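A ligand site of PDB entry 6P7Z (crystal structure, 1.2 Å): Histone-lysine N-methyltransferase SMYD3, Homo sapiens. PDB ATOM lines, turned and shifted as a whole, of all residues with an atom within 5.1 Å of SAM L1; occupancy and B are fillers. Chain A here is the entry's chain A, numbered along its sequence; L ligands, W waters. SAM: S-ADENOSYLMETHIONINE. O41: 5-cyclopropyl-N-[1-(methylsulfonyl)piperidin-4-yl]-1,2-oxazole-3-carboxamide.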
ATOM      1  N   ASN A  17      16.546  -5.493  17.306  1.00  0.00           N
ATOM      2  CA  ASN A  17      16.329  -6.054  18.649  1.00  0.00           C
ATOM      3  C   ASN A  17      16.665  -7.529  18.770  1.00  0.00           C
ATOM      4  O   ASN A  17      16.242  -8.167  19.746  1.00  0.00           O
ATOM      5  CB  ASN A  17      14.893  -5.792  19.158  1.00  0.00           C
ATOM      6  CG  ASN A  17      13.831  -6.342  18.236  1.00  0.00           C
ATOM      7  OD1 ASN A  17      13.983  -7.396  17.643  1.00  0.00           O
ATOM      8  ND2 ASN A  17      12.723  -5.619  18.133  1.00  0.00           N
ATOM      9  N   ARG A  18      17.413  -8.095  17.824  1.00  0.00           N
ATOM     10  CA  ARG A  18      17.775  -9.510  17.876  1.00  0.00           C
ATOM     11  C   ARG A  18      19.280  -9.723  17.769  1.00  0.00           C
ATOM     12  O   ARG A  18      19.700 -10.836  17.453  1.00  0.00           O
ATOM     13  CB  ARG A  18      17.091 -10.316  16.772  1.00  0.00           C
ATOM     14  CG  ARG A  18      15.608 -10.151  16.629  1.00  0.00           C
ATOM     15  CD  ARG A  18      15.134 -10.874  15.384  1.00  0.00           C
ATOM     16  NE  ARG A  18      13.685 -10.916  15.307  1.00  0.00           N
ATOM     17  CZ  ARG A  18      12.996 -11.290  14.241  1.00  0.00           C
ATOM     18  NH1 ARG A  18      13.633 -11.651  13.131  1.00  0.00           N
ATOM     19  NH2 ARG A  18      11.675 -11.300  14.265  1.00  0.00           N
ATOM     20  N   GLY A  19      20.087  -8.691  17.992  1.00  0.00           N
ATOM     21  CA  GLY A  19      21.514  -8.821  17.766  1.00  0.00           C
ATOM     22  C   GLY A  19      21.860  -8.758  16.282  1.00  0.00           C
ATOM     23  O   GLY A  19      21.211  -8.070  15.497  1.00  0.00           O
ATOM     24  N   ASN A  20      22.916  -9.472  15.892  1.00  0.00           N
ATOM     25  CA  ASN A  20      23.241  -9.567  14.490  1.00  0.00           C
ATOM     26  C   ASN A  20      22.299 -10.554  13.804  1.00  0.00           C
ATOM     27  O   ASN A  20      21.676 -11.405  14.443  1.00  0.00           O
ATOM     28  CB  ASN A  20      24.689  -9.997  14.318  1.00  0.00           C
ATOM     29  CG  ASN A  20      25.646  -8.945  14.817  1.00  0.00           C
ATOM     30  OD1 ASN A  20      25.476  -7.766  14.527  1.00  0.00           O
ATOM     31  ND2 ASN A  20      26.627  -9.360  15.614  1.00  0.00           N
ATOM     32  N   GLY A  21      22.185 -10.408  12.487  1.00  0.00           N
ATOM     33  CA  GLY A  21      21.369 -11.294  11.680  1.00  0.00           C
ATOM     34  C   GLY A  21      21.908 -11.361  10.273  1.00  0.00           C
ATOM     35  O   GLY A  21      22.949 -10.802   9.961  1.00  0.00           O
ATOM     36  N   TYR A 128      31.169 -14.712   9.999  1.00  0.00           N
ATOM     37  CA  TYR A 128      31.017 -14.580  11.443  1.00  0.00           C
ATOM     38  C   TYR A 128      31.862 -15.684  12.047  1.00  0.00           C
ATOM     39  O   TYR A 128      31.852 -16.810  11.541  1.00  0.00           O
ATOM     40  CB  TYR A 128      29.558 -14.832  11.827  1.00  0.00           C
ATOM     41  CG  TYR A 128      28.968 -14.131  13.043  1.00  0.00           C
ATOM     42  CD1 TYR A 128      29.174 -12.782  13.290  1.00  0.00           C
ATOM     43  CD2 TYR A 128      28.122 -14.833  13.900  1.00  0.00           C
ATOM     44  CE1 TYR A 128      28.562 -12.152  14.378  1.00  0.00           C
ATOM     45  CE2 TYR A 128      27.514 -14.215  14.981  1.00  0.00           C
ATOM     46  CZ  TYR A 128      27.741 -12.876  15.211  1.00  0.00           C
ATOM     47  OH  TYR A 128      27.111 -12.260  16.262  1.00  0.00           O
ATOM     48  N   ASP A 132      33.007 -14.122  17.498  1.00  0.00           N
ATOM     49  CA  ASP A 132      31.876 -13.199  17.375  1.00  0.00           C
ATOM     50  C   ASP A 132      30.574 -13.734  17.952  1.00  0.00           C
ATOM     51  O   ASP A 132      29.631 -12.939  18.142  1.00  0.00           O
ATOM     52  CB  ASP A 132      31.579 -12.916  15.894  1.00  0.00           C
ATOM     53  CG  ASP A 132      32.732 -12.255  15.144  1.00  0.00           C
ATOM     54  OD1 ASP A 132      33.400 -11.360  15.721  1.00  0.00           O
ATOM     55  OD2 ASP A 132      32.932 -12.609  13.962  1.00  0.00           O
ATOM     56  N   LEU A 133      30.466 -15.029  18.187  1.00  0.00           N
ATOM     57  CA  LEU A 133      29.178 -15.645  18.475  1.00  0.00           C
ATOM     58  C   LEU A 133      28.541 -15.051  19.729  1.00  0.00           C
ATOM     59  O   LEU A 133      29.228 -14.661  20.677  1.00  0.00           O
ATOM     60  CB  LEU A 133      29.318 -17.141  18.673  1.00  0.00           C
ATOM     61  CG  LEU A 133      29.721 -17.950  17.444  1.00  0.00           C
ATOM     62  CD1 LEU A 133      29.932 -19.400  17.822  1.00  0.00           C
ATOM     63  CD2 LEU A 133      28.676 -17.831  16.348  1.00  0.00           C
ATOM     64  N   GLU A 134      27.214 -15.029  19.726  1.00  0.00           N
ATOM     65  CA  GLU A 134      26.445 -14.606  20.888  1.00  0.00           C
ATOM     66  C   GLU A 134      26.629 -15.567  22.048  1.00  0.00           C
ATOM     67  O   GLU A 134      26.519 -16.789  21.880  1.00  0.00           O
ATOM     68  CB  GLU A 134      24.964 -14.555  20.510  1.00  0.00           C
ATOM     69  CG  GLU A 134      24.046 -14.152  21.660  1.00  0.00           C
ATOM     70  CD  GLU A 134      24.306 -12.739  22.112  1.00  0.00           C
ATOM     71  OE1 GLU A 134      23.917 -11.808  21.366  1.00  0.00           O
ATOM     72  OE2 GLU A 134      24.921 -12.554  23.187  1.00  0.00           O
ATOM     73  N   ASN A 136      25.051 -14.577  25.252  1.00  0.00           N
ATOM     74  CA  ASN A 136      23.946 -14.292  26.148  1.00  0.00           C
ATOM     75  C   ASN A 136      24.334 -14.287  27.623  1.00  0.00           C
ATOM     76  O   ASN A 136      23.504 -14.540  28.490  1.00  0.00           O
ATOM     77  CB  ASN A 136      22.766 -15.230  25.913  1.00  0.00           C
ATOM     78  CG  ASN A 136      22.051 -14.919  24.625  1.00  0.00           C
ATOM     79  OD1 ASN A 136      21.780 -13.763  24.327  1.00  0.00           O
ATOM     80  ND2 ASN A 136      21.775 -15.952  23.838  1.00  0.00           N
ATOM     81  N   CYS A 184      24.037 -21.785  22.821  1.00  0.00           N
ATOM     82  CA  CYS A 184      23.076 -21.136  21.947  1.00  0.00           C
ATOM     83  C   CYS A 184      23.489 -21.132  20.476  1.00  0.00           C
ATOM     84  O   CYS A 184      22.809 -20.504  19.646  1.00  0.00           O
ATOM     85  CB  CYS A 184      22.719 -19.715  22.418  1.00  0.00           C
ATOM     86  SG  CYS A 184      24.056 -18.504  22.533  1.00  0.00           S
ATOM     87  N   ASN A 185      24.583 -21.822  20.130  1.00  0.00           N
ATOM     88  CA  ASN A 185      25.007 -21.863  18.738  1.00  0.00           C
ATOM     89  C   ASN A 185      25.291 -23.260  18.200  1.00  0.00           C
ATOM     90  O   ASN A 185      25.735 -23.374  17.055  1.00  0.00           O
ATOM     91  CB  ASN A 185      26.212 -20.945  18.505  1.00  0.00           C
ATOM     92  CG  ASN A 185      25.890 -19.498  18.725  1.00  0.00           C
ATOM     93  OD1 ASN A 185      25.266 -18.844  17.868  1.00  0.00           O
ATOM     94  ND2 ASN A 185      26.281 -18.969  19.871  1.00  0.00           N
ATOM     95  N   SER A 206      25.352 -19.319  12.059  1.00  0.00           N
ATOM     96  CA  SER A 206      24.851 -18.827  13.324  1.00  0.00           C
ATOM     97  C   SER A 206      24.340 -17.403  13.250  1.00  0.00           C
ATOM     98  O   SER A 206      23.720 -16.950  14.208  1.00  0.00           O
ATOM     99  CB  SER A 206      25.918 -18.910  14.404  1.00  0.00           C
ATOM    100  OG  SER A 206      25.990 -20.220  14.944  1.00  0.00           O
ATOM    101  N   LEU A 207      24.562 -16.687  12.145  1.00  0.00           N
ATOM    102  CA  LEU A 207      23.943 -15.367  12.023  1.00  0.00           C
ATOM    103  C   LEU A 207      22.427 -15.437  11.892  1.00  0.00           C
ATOM    104  O   LEU A 207      21.766 -14.425  12.161  1.00  0.00           O
ATOM    105  CB  LEU A 207      24.505 -14.626  10.812  1.00  0.00           C
ATOM    106  CG  LEU A 207      25.842 -13.948  11.072  1.00  0.00           C
ATOM    107  CD1 LEU A 207      26.491 -13.514   9.765  1.00  0.00           C
ATOM    108  CD2 LEU A 207      25.696 -12.771  12.037  1.00  0.00           C
ATOM    109  N   LEU A 208      21.865 -16.580  11.506  1.00  0.00           N
ATOM    110  CA  LEU A 208      20.429 -16.649  11.254  1.00  0.00           C
ATOM    111  C   LEU A 208      19.643 -16.593  12.567  1.00  0.00           C
ATOM    112  O   LEU A 208      19.808 -17.463  13.420  1.00  0.00           O
ATOM    113  CB  LEU A 208      20.081 -17.946  10.543  1.00  0.00           C
ATOM    114  CG  LEU A 208      20.585 -18.031   9.099  1.00  0.00           C
ATOM    115  CD1 LEU A 208      20.771 -19.477   8.694  1.00  0.00           C
ATOM    116  CD2 LEU A 208      19.613 -17.346   8.169  1.00  0.00           C
ATOM    117  N   ASN A 209      18.739 -15.637  12.662  1.00  0.00           N
ATOM    118  CA  ASN A 209      17.803 -15.616  13.772  1.00  0.00           C
ATOM    119  C   ASN A 209      16.648 -16.587  13.536  1.00  0.00           C
ATOM    120  O   ASN A 209      16.443 -17.108  12.436  1.00  0.00           O
ATOM    121  CB  ASN A 209      17.339 -14.184  14.030  1.00  0.00           C
ATOM    122  CG  ASN A 209      18.444 -13.363  14.651  1.00  0.00           C
ATOM    123  OD1 ASN A 209      19.101 -13.806  15.592  1.00  0.00           O
ATOM    124  ND2 ASN A 209      18.682 -12.176  14.113  1.00  0.00           N
ATOM    125  N   HIS A 210      15.921 -16.857  14.609  1.00  0.00           N
ATOM    126  CA  HIS A 210      14.867 -17.849  14.644  1.00  0.00           C
ATOM    127  C   HIS A 210      13.518 -17.263  14.276  1.00  0.00           C
ATOM    128  O   HIS A 210      13.188 -16.124  14.662  1.00  0.00           O
ATOM    129  CB  HIS A 210      14.758 -18.408  16.069  1.00  0.00           C
ATOM    130  CG  HIS A 210      13.499 -19.155  16.311  1.00  0.00           C
ATOM    131  ND1 HIS A 210      13.336 -20.488  15.995  1.00  0.00           N
ATOM    132  CD2 HIS A 210      12.300 -18.735  16.802  1.00  0.00           C
ATOM    133  CE1 HIS A 210      12.108 -20.862  16.308  1.00  0.00           C
ATOM    134  NE2 HIS A 210      11.454 -19.811  16.774  1.00  0.00           N
ATOM    135  N   SER A 211      12.715 -18.061  13.589  1.00  0.00           N
ATOM    136  CA  SER A 211      11.290 -17.814  13.456  1.00  0.00           C
ATOM    137  C   SER A 211      10.547 -19.127  13.553  1.00  0.00           C
ATOM    138  O   SER A 211      11.025 -20.156  13.053  1.00  0.00           O
ATOM    139  CB  SER A 211      10.975 -17.151  12.113  1.00  0.00           C
ATOM    140  OG  SER A 211       9.567 -17.110  11.936  1.00  0.00           O
ATOM    141  N   TYR A 243      14.693 -22.797  14.721  1.00  0.00           N
ATOM    142  CA  TYR A 243      15.661 -23.550  15.509  1.00  0.00           C
ATOM    143  C   TYR A 243      15.087 -24.865  16.023  1.00  0.00           C
ATOM    144  O   TYR A 243      15.861 -25.724  16.447  1.00  0.00           O
ATOM    145  CB  TYR A 243      16.106 -22.745  16.726  1.00  0.00           C
ATOM    146  CG  TYR A 243      16.876 -21.471  16.458  1.00  0.00           C
ATOM    147  CD1 TYR A 243      17.241 -21.078  15.178  1.00  0.00           C
ATOM    148  CD2 TYR A 243      17.261 -20.676  17.528  1.00  0.00           C
ATOM    149  CE1 TYR A 243      17.970 -19.897  14.974  1.00  0.00           C
ATOM    150  CE2 TYR A 243      17.975 -19.511  17.332  1.00  0.00           C
ATOM    151  CZ  TYR A 243      18.317 -19.124  16.072  1.00  0.00           C
ATOM    152  OH  TYR A 243      19.040 -17.956  15.912  1.00  0.00           O
ATOM    153  N   TYR A 261      18.189 -20.362  24.400  1.00  0.00           N
ATOM    154  CA  TYR A 261      18.497 -19.230  23.546  1.00  0.00           C
ATOM    155  C   TYR A 261      18.280 -17.869  24.194  1.00  0.00           C
ATOM    156  O   TYR A 261      18.557 -16.844  23.558  1.00  0.00           O
ATOM    157  CB  TYR A 261      17.723 -19.331  22.224  1.00  0.00           C
ATOM    158  CG  TYR A 261      18.087 -20.571  21.438  1.00  0.00           C
ATOM    159  CD1 TYR A 261      19.311 -20.651  20.772  1.00  0.00           C
ATOM    160  CD2 TYR A 261      17.235 -21.661  21.383  1.00  0.00           C
ATOM    161  CE1 TYR A 261      19.661 -21.781  20.072  1.00  0.00           C
ATOM    162  CE2 TYR A 261      17.589 -22.806  20.663  1.00  0.00           C
ATOM    163  CZ  TYR A 261      18.802 -22.846  20.027  1.00  0.00           C
ATOM    164  OH  TYR A 261      19.145 -23.971  19.311  1.00  0.00           O
ATOM    165  N   CYS A 262      17.766 -17.831  25.421  1.00  0.00           N
ATOM    166  CA  CYS A 262      17.583 -16.582  26.151  1.00  0.00           C
ATOM    167  C   CYS A 262      16.803 -15.523  25.359  1.00  0.00           C
ATOM    168  O   CYS A 262      17.190 -14.355  25.324  1.00  0.00           O
ATOM    169  CB  CYS A 262      18.918 -16.009  26.625  1.00  0.00           C
ATOM    170  SG  CYS A 262      19.750 -17.022  27.818  1.00  0.00           S
ATOM    171  N   PHE A 263      15.701 -15.913  24.728  1.00  0.00           N
ATOM    172  CA  PHE A 263      14.826 -14.874  24.186  1.00  0.00           C
ATOM    173  C   PHE A 263      13.375 -15.296  24.262  1.00  0.00           C
ATOM    174  O   PHE A 263      13.051 -16.467  24.440  1.00  0.00           O
ATOM    175  CB  PHE A 263      15.193 -14.402  22.775  1.00  0.00           C
ATOM    176  CG  PHE A 263      14.861 -15.387  21.683  1.00  0.00           C
ATOM    177  CD1 PHE A 263      15.763 -16.388  21.335  1.00  0.00           C
ATOM    178  CD2 PHE A 263      13.657 -15.310  20.985  1.00  0.00           C
ATOM    179  CE1 PHE A 263      15.470 -17.282  20.315  1.00  0.00           C
ATOM    180  CE2 PHE A 263      13.360 -16.210  19.957  1.00  0.00           C
ATOM    181  CZ  PHE A 263      14.269 -17.197  19.637  1.00  0.00           C
ATOM    182  N   GLU A 264      12.496 -14.285  24.146  1.00  0.00           N
ATOM    183  CA  GLU A 264      11.047 -14.419  24.137  1.00  0.00           C
ATOM    184  C   GLU A 264      10.566 -14.178  22.715  1.00  0.00           C
ATOM    185  O   GLU A 264      10.902 -13.157  22.106  1.00  0.00           O
ATOM    186  CB  GLU A 264      10.413 -13.350  25.046  1.00  0.00           C
ATOM    187  CG  GLU A 264      11.160 -13.084  26.352  1.00  0.00           C
ATOM    188  CD  GLU A 264      11.121 -14.271  27.303  1.00  0.00           C
ATOM    189  OE1 GLU A 264      11.872 -14.256  28.305  1.00  0.00           O
ATOM    190  OE2 GLU A 264      10.344 -15.226  27.067  1.00  0.00           O
ATOM    191  N   CYS A 265       9.833 -15.128  22.153  1.00  0.00           N
ATOM    192  CA  CYS A 265       9.450 -15.050  20.746  1.00  0.00           C
ATOM    193  C   CYS A 265       8.159 -14.270  20.597  1.00  0.00           C
ATOM    194  O   CYS A 265       7.147 -14.597  21.241  1.00  0.00           O
ATOM    195  CB  CYS A 265       9.271 -16.418  20.089  1.00  0.00           C
ATOM    196  SG  CYS A 265       9.172 -16.390  18.265  1.00  0.00           S
HETATM  197  N   SAM L   1      21.439 -12.757  16.899  1.00  0.00           N
HETATM  198  CA  SAM L   1      22.573 -13.694  16.945  1.00  0.00           C
HETATM  199  C   SAM L   1      23.906 -12.963  17.055  1.00  0.00           C
HETATM  200  O   SAM L   1      24.955 -13.611  16.979  1.00  0.00           O
HETATM  201  OXT SAM L   1      23.876 -11.729  17.236  1.00  0.00           O
HETATM  202  CB  SAM L   1      22.526 -14.652  15.763  1.00  0.00           C
HETATM  203  CG  SAM L   1      21.622 -15.864  16.025  1.00  0.00           C
HETATM  204  SD  SAM L   1      22.348 -16.951  17.289  1.00  0.00           S
HETATM  205  CE  SAM L   1      22.327 -18.569  16.498  1.00  0.00           C
HETATM  206  C5' SAM L   1      20.983 -17.152  18.484  1.00  0.00           C
HETATM  207  C4' SAM L   1      20.705 -15.947  19.354  1.00  0.00           C
HETATM  208  O4' SAM L   1      20.141 -14.919  18.564  1.00  0.00           O
HETATM  209  C3' SAM L   1      19.669 -16.216  20.432  1.00  0.00           C
HETATM  210  O3' SAM L   1      20.272 -16.851  21.535  1.00  0.00           O
HETATM  211  C2' SAM L   1      19.143 -14.824  20.689  1.00  0.00           C
HETATM  212  O2' SAM L   1      20.125 -14.088  21.416  1.00  0.00           O
HETATM  213  C1' SAM L   1      19.104 -14.275  19.286  1.00  0.00           C
HETATM  214  N9  SAM L   1      17.842 -14.545  18.568  1.00  0.00           N
HETATM  215  C8  SAM L   1      17.653 -15.483  17.570  1.00  0.00           C
HETATM  216  N7  SAM L   1      16.388 -15.418  17.125  1.00  0.00           N
HETATM  217  C5  SAM L   1      15.755 -14.442  17.824  1.00  0.00           C
HETATM  218  C6  SAM L   1      14.454 -13.933  17.807  1.00  0.00           C
HETATM  219  N6  SAM L   1      13.490 -14.367  16.973  1.00  0.00           N
HETATM  220  N1  SAM L   1      14.134 -12.917  18.667  1.00  0.00           N
HETATM  221  C2  SAM L   1      15.074 -12.423  19.549  1.00  0.00           C
HETATM  222  N3  SAM L   1      16.354 -12.903  19.596  1.00  0.00           N
HETATM  223  C4  SAM L   1      16.661 -13.889  18.731  1.00  0.00           C
HETATM  224  C10 O41 L   2      15.521 -28.650  13.583  1.00  0.00           C
HETATM  225  C15 O41 L   2      20.350 -24.742  15.644  1.00  0.00           C
HETATM  226  C20 O41 L   2      22.270 -22.451  16.234  1.00  0.00           C
HETATM  227  C21 O41 L   2      21.070 -21.984  16.991  1.00  0.00           C
HETATM  228  C01 O41 L   2      14.803 -29.442   9.746  1.00  0.00           C
HETATM  229  C06 O41 L   2      17.181 -30.276  12.705  1.00  0.00           C
HETATM  230  C07 O41 L   2      18.278 -29.638  13.570  1.00  0.00           C
HETATM  231  C08 O41 L   2      17.689 -28.919  14.799  1.00  0.00           C
HETATM  232  C09 O41 L   2      16.163 -29.064  14.920  1.00  0.00           C
HETATM  233  C12 O41 L   2      19.170 -27.037  15.047  1.00  0.00           C
HETATM  234  C14 O41 L   2      19.438 -25.607  14.875  1.00  0.00           C
HETATM  235  C16 O41 L   2      20.235 -23.526  15.110  1.00  0.00           C
HETATM  236  C19 O41 L   2      20.959 -22.280  15.542  1.00  0.00           C
HETATM  237  N05 O41 L   2      15.988 -29.456  12.446  1.00  0.00           N
HETATM  238  N11 O41 L   2      17.993 -27.501  14.661  1.00  0.00           N
HETATM  239  N18 O41 L   2      18.857 -24.862  13.939  1.00  0.00           N
HETATM  240  O03 O41 L   2      15.024 -31.564  11.332  1.00  0.00           O
HETATM  241  O04 O41 L   2      13.489 -29.924  11.990  1.00  0.00           O
HETATM  242  O13 O41 L   2      20.020 -27.800  15.516  1.00  0.00           O
HETATM  243  O17 O41 L   2      19.327 -23.563  14.061  1.00  0.00           O
HETATM  244  S02 O41 L   2      14.775 -30.158  11.413  1.00  0.00           S
HETATM  245  O   HOH W   1      11.483 -12.142  19.547  1.00  0.00           O
HETATM  246  O   HOH W   2      10.560 -13.757  16.929  1.00  0.00           O
HETATM  247  O   HOH W   3      21.530 -19.756  13.390  1.00  0.00           O
HETATM  248  O   HOH W   4      21.627 -12.171  19.808  1.00  0.00           O
HETATM  249  O   HOH W   5      18.883 -13.187  23.647  1.00  0.00           O
HETATM  250  O   HOH W   6      25.454 -10.747  19.200  1.00  0.00           O
HETATM  251  O   HOH W   7      25.852 -16.181  17.554  1.00  0.00           O
HETATM  252  O   HOH W   8      17.519 -11.445  21.740  1.00  0.00           O
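The backbone carbonyl oxygen (O) of Glu 134 sits at hydrogen-bond distance from the side-chain sulfur (SG) of Cys 184.
The side-chain amide nitrogen (ND2) of Asn 136 is in hydrogen-bond range of the side-chain sulfur (SG) of Cys 184 (3.7 Å).
The side-chain amide nitrogen (ND2) of Asn 185 sits at hydrogen-bond distance from the side-chain sulfur (SG) of Cys 184 (3.5 Å).
The backbone NH (N) of Asn 136 lies within hydrogen-bond range of the side-chain carboxylate (OE2) of Glu 134, at 2.9 Å.
A ring nitrogen (ND1) of His 210 sits at hydrogen-bond distance from the backbone NH of Tyr 243.
The backbone carbonyl oxygen (O) of Asp 132 is in hydrogen-bond range of the side-chain hydroxyl (OH) of Tyr 128 (3.2 Å).
The backbone carbonyl oxygen (O) of Asn 20 lies within hydrogen-bond range of the side-chain amide nitrogen (ND2) of Asn 209.
The side-chain hydroxyl (OH) of Tyr 243 is in hydrogen-bond range of the backbone carbonyl oxygen (O) of Leu 208.
OD1 of Asn 209 lies within hydrogen-bond range of N of SAM L1 (2.9 Å).
The side-chain hydroxyl (OH) of Tyr 128 lies within hydrogen-bond range of an oxygen (O) of SAM L1, 2.6 Å away.
N of SAM L1 lies within hydrogen-bond range of O of Asn 20, 2.8 Å away.
O of Tyr 261 is in hydrogen-bond range of O3' of SAM L1 (2.7 Å).
A nitrogen (N) of SAM L1 sits at hydrogen-bond distance from the backbone carbonyl oxygen (O) of Arg 18.
O of Tyr 243 lies within hydrogen-bond range of N11 of O41 L2 (3.3 Å).
O of His 210 is in hydrogen-bond range of N6 of SAM L1 (2.9 Å).
The side-chain amide nitrogen (ND2) of Asn 136 lies within hydrogen-bond range of an oxygen (O3') of SAM L1, at 2.9 Å.
A nitrogen (N7) of SAM L1 is in hydrogen-bond range of the backbone NH of His 210.
An oxygen (OXT) of SAM L1 lies within hydrogen-bond range of the backbone NH (N) of Asn 20.
Water W6 lies within hydrogen-bond range of OXT of SAM L1 and OE1 of Glu 134.
Water W5 lies within hydrogen-bond range of the backbone carbonyl oxygen of Cys 262 (2.7 Å), an oxygen (O2') of SAM L1 (2.7 Å) and the side-chain amide oxygen of Asn 136 (3.0 Å).
Water W7 lies within hydrogen-bond range of OD1 of Asn 185 (2.7 Å), O of SAM L1 (2.8 Å) and N of Glu 134 (2.8 Å).
Water W1 bridges the backbone carbonyl oxygen of Glu 264 and a nitrogen (N1) of SAM L1.
Water W4 lies within hydrogen-bond range of the side-chain carboxylate (OE1) of Glu 134 (2.8 Å), an oxygen (O2') of SAM L1 (2.9 Å) and the backbone carbonyl oxygen (O) of Arg 18 (3.3 Å).
The side-chain amide oxygen (OD1) of Asn 185 lies close to a sulfur (SD) of SAM L1, at 3.5 Å.
O of Ser 206 lies close to SD of SAM L1, 3.4 Å away.
The side-chain hydroxyl (OH) of Tyr 243 sits close to a sulfur (SD) of SAM L1 (3.7 Å).
Gly 19 touches SAM L1 (C to OXT, 3.7 Å).
Glu 134 touches SAM L1.
Cys 184 touches SAM L1 (O to CE, 3.7 Å).
Leu 207 touches SAM L1.
Leu 208 touches SAM L1.
Phe 263 touches SAM L1.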
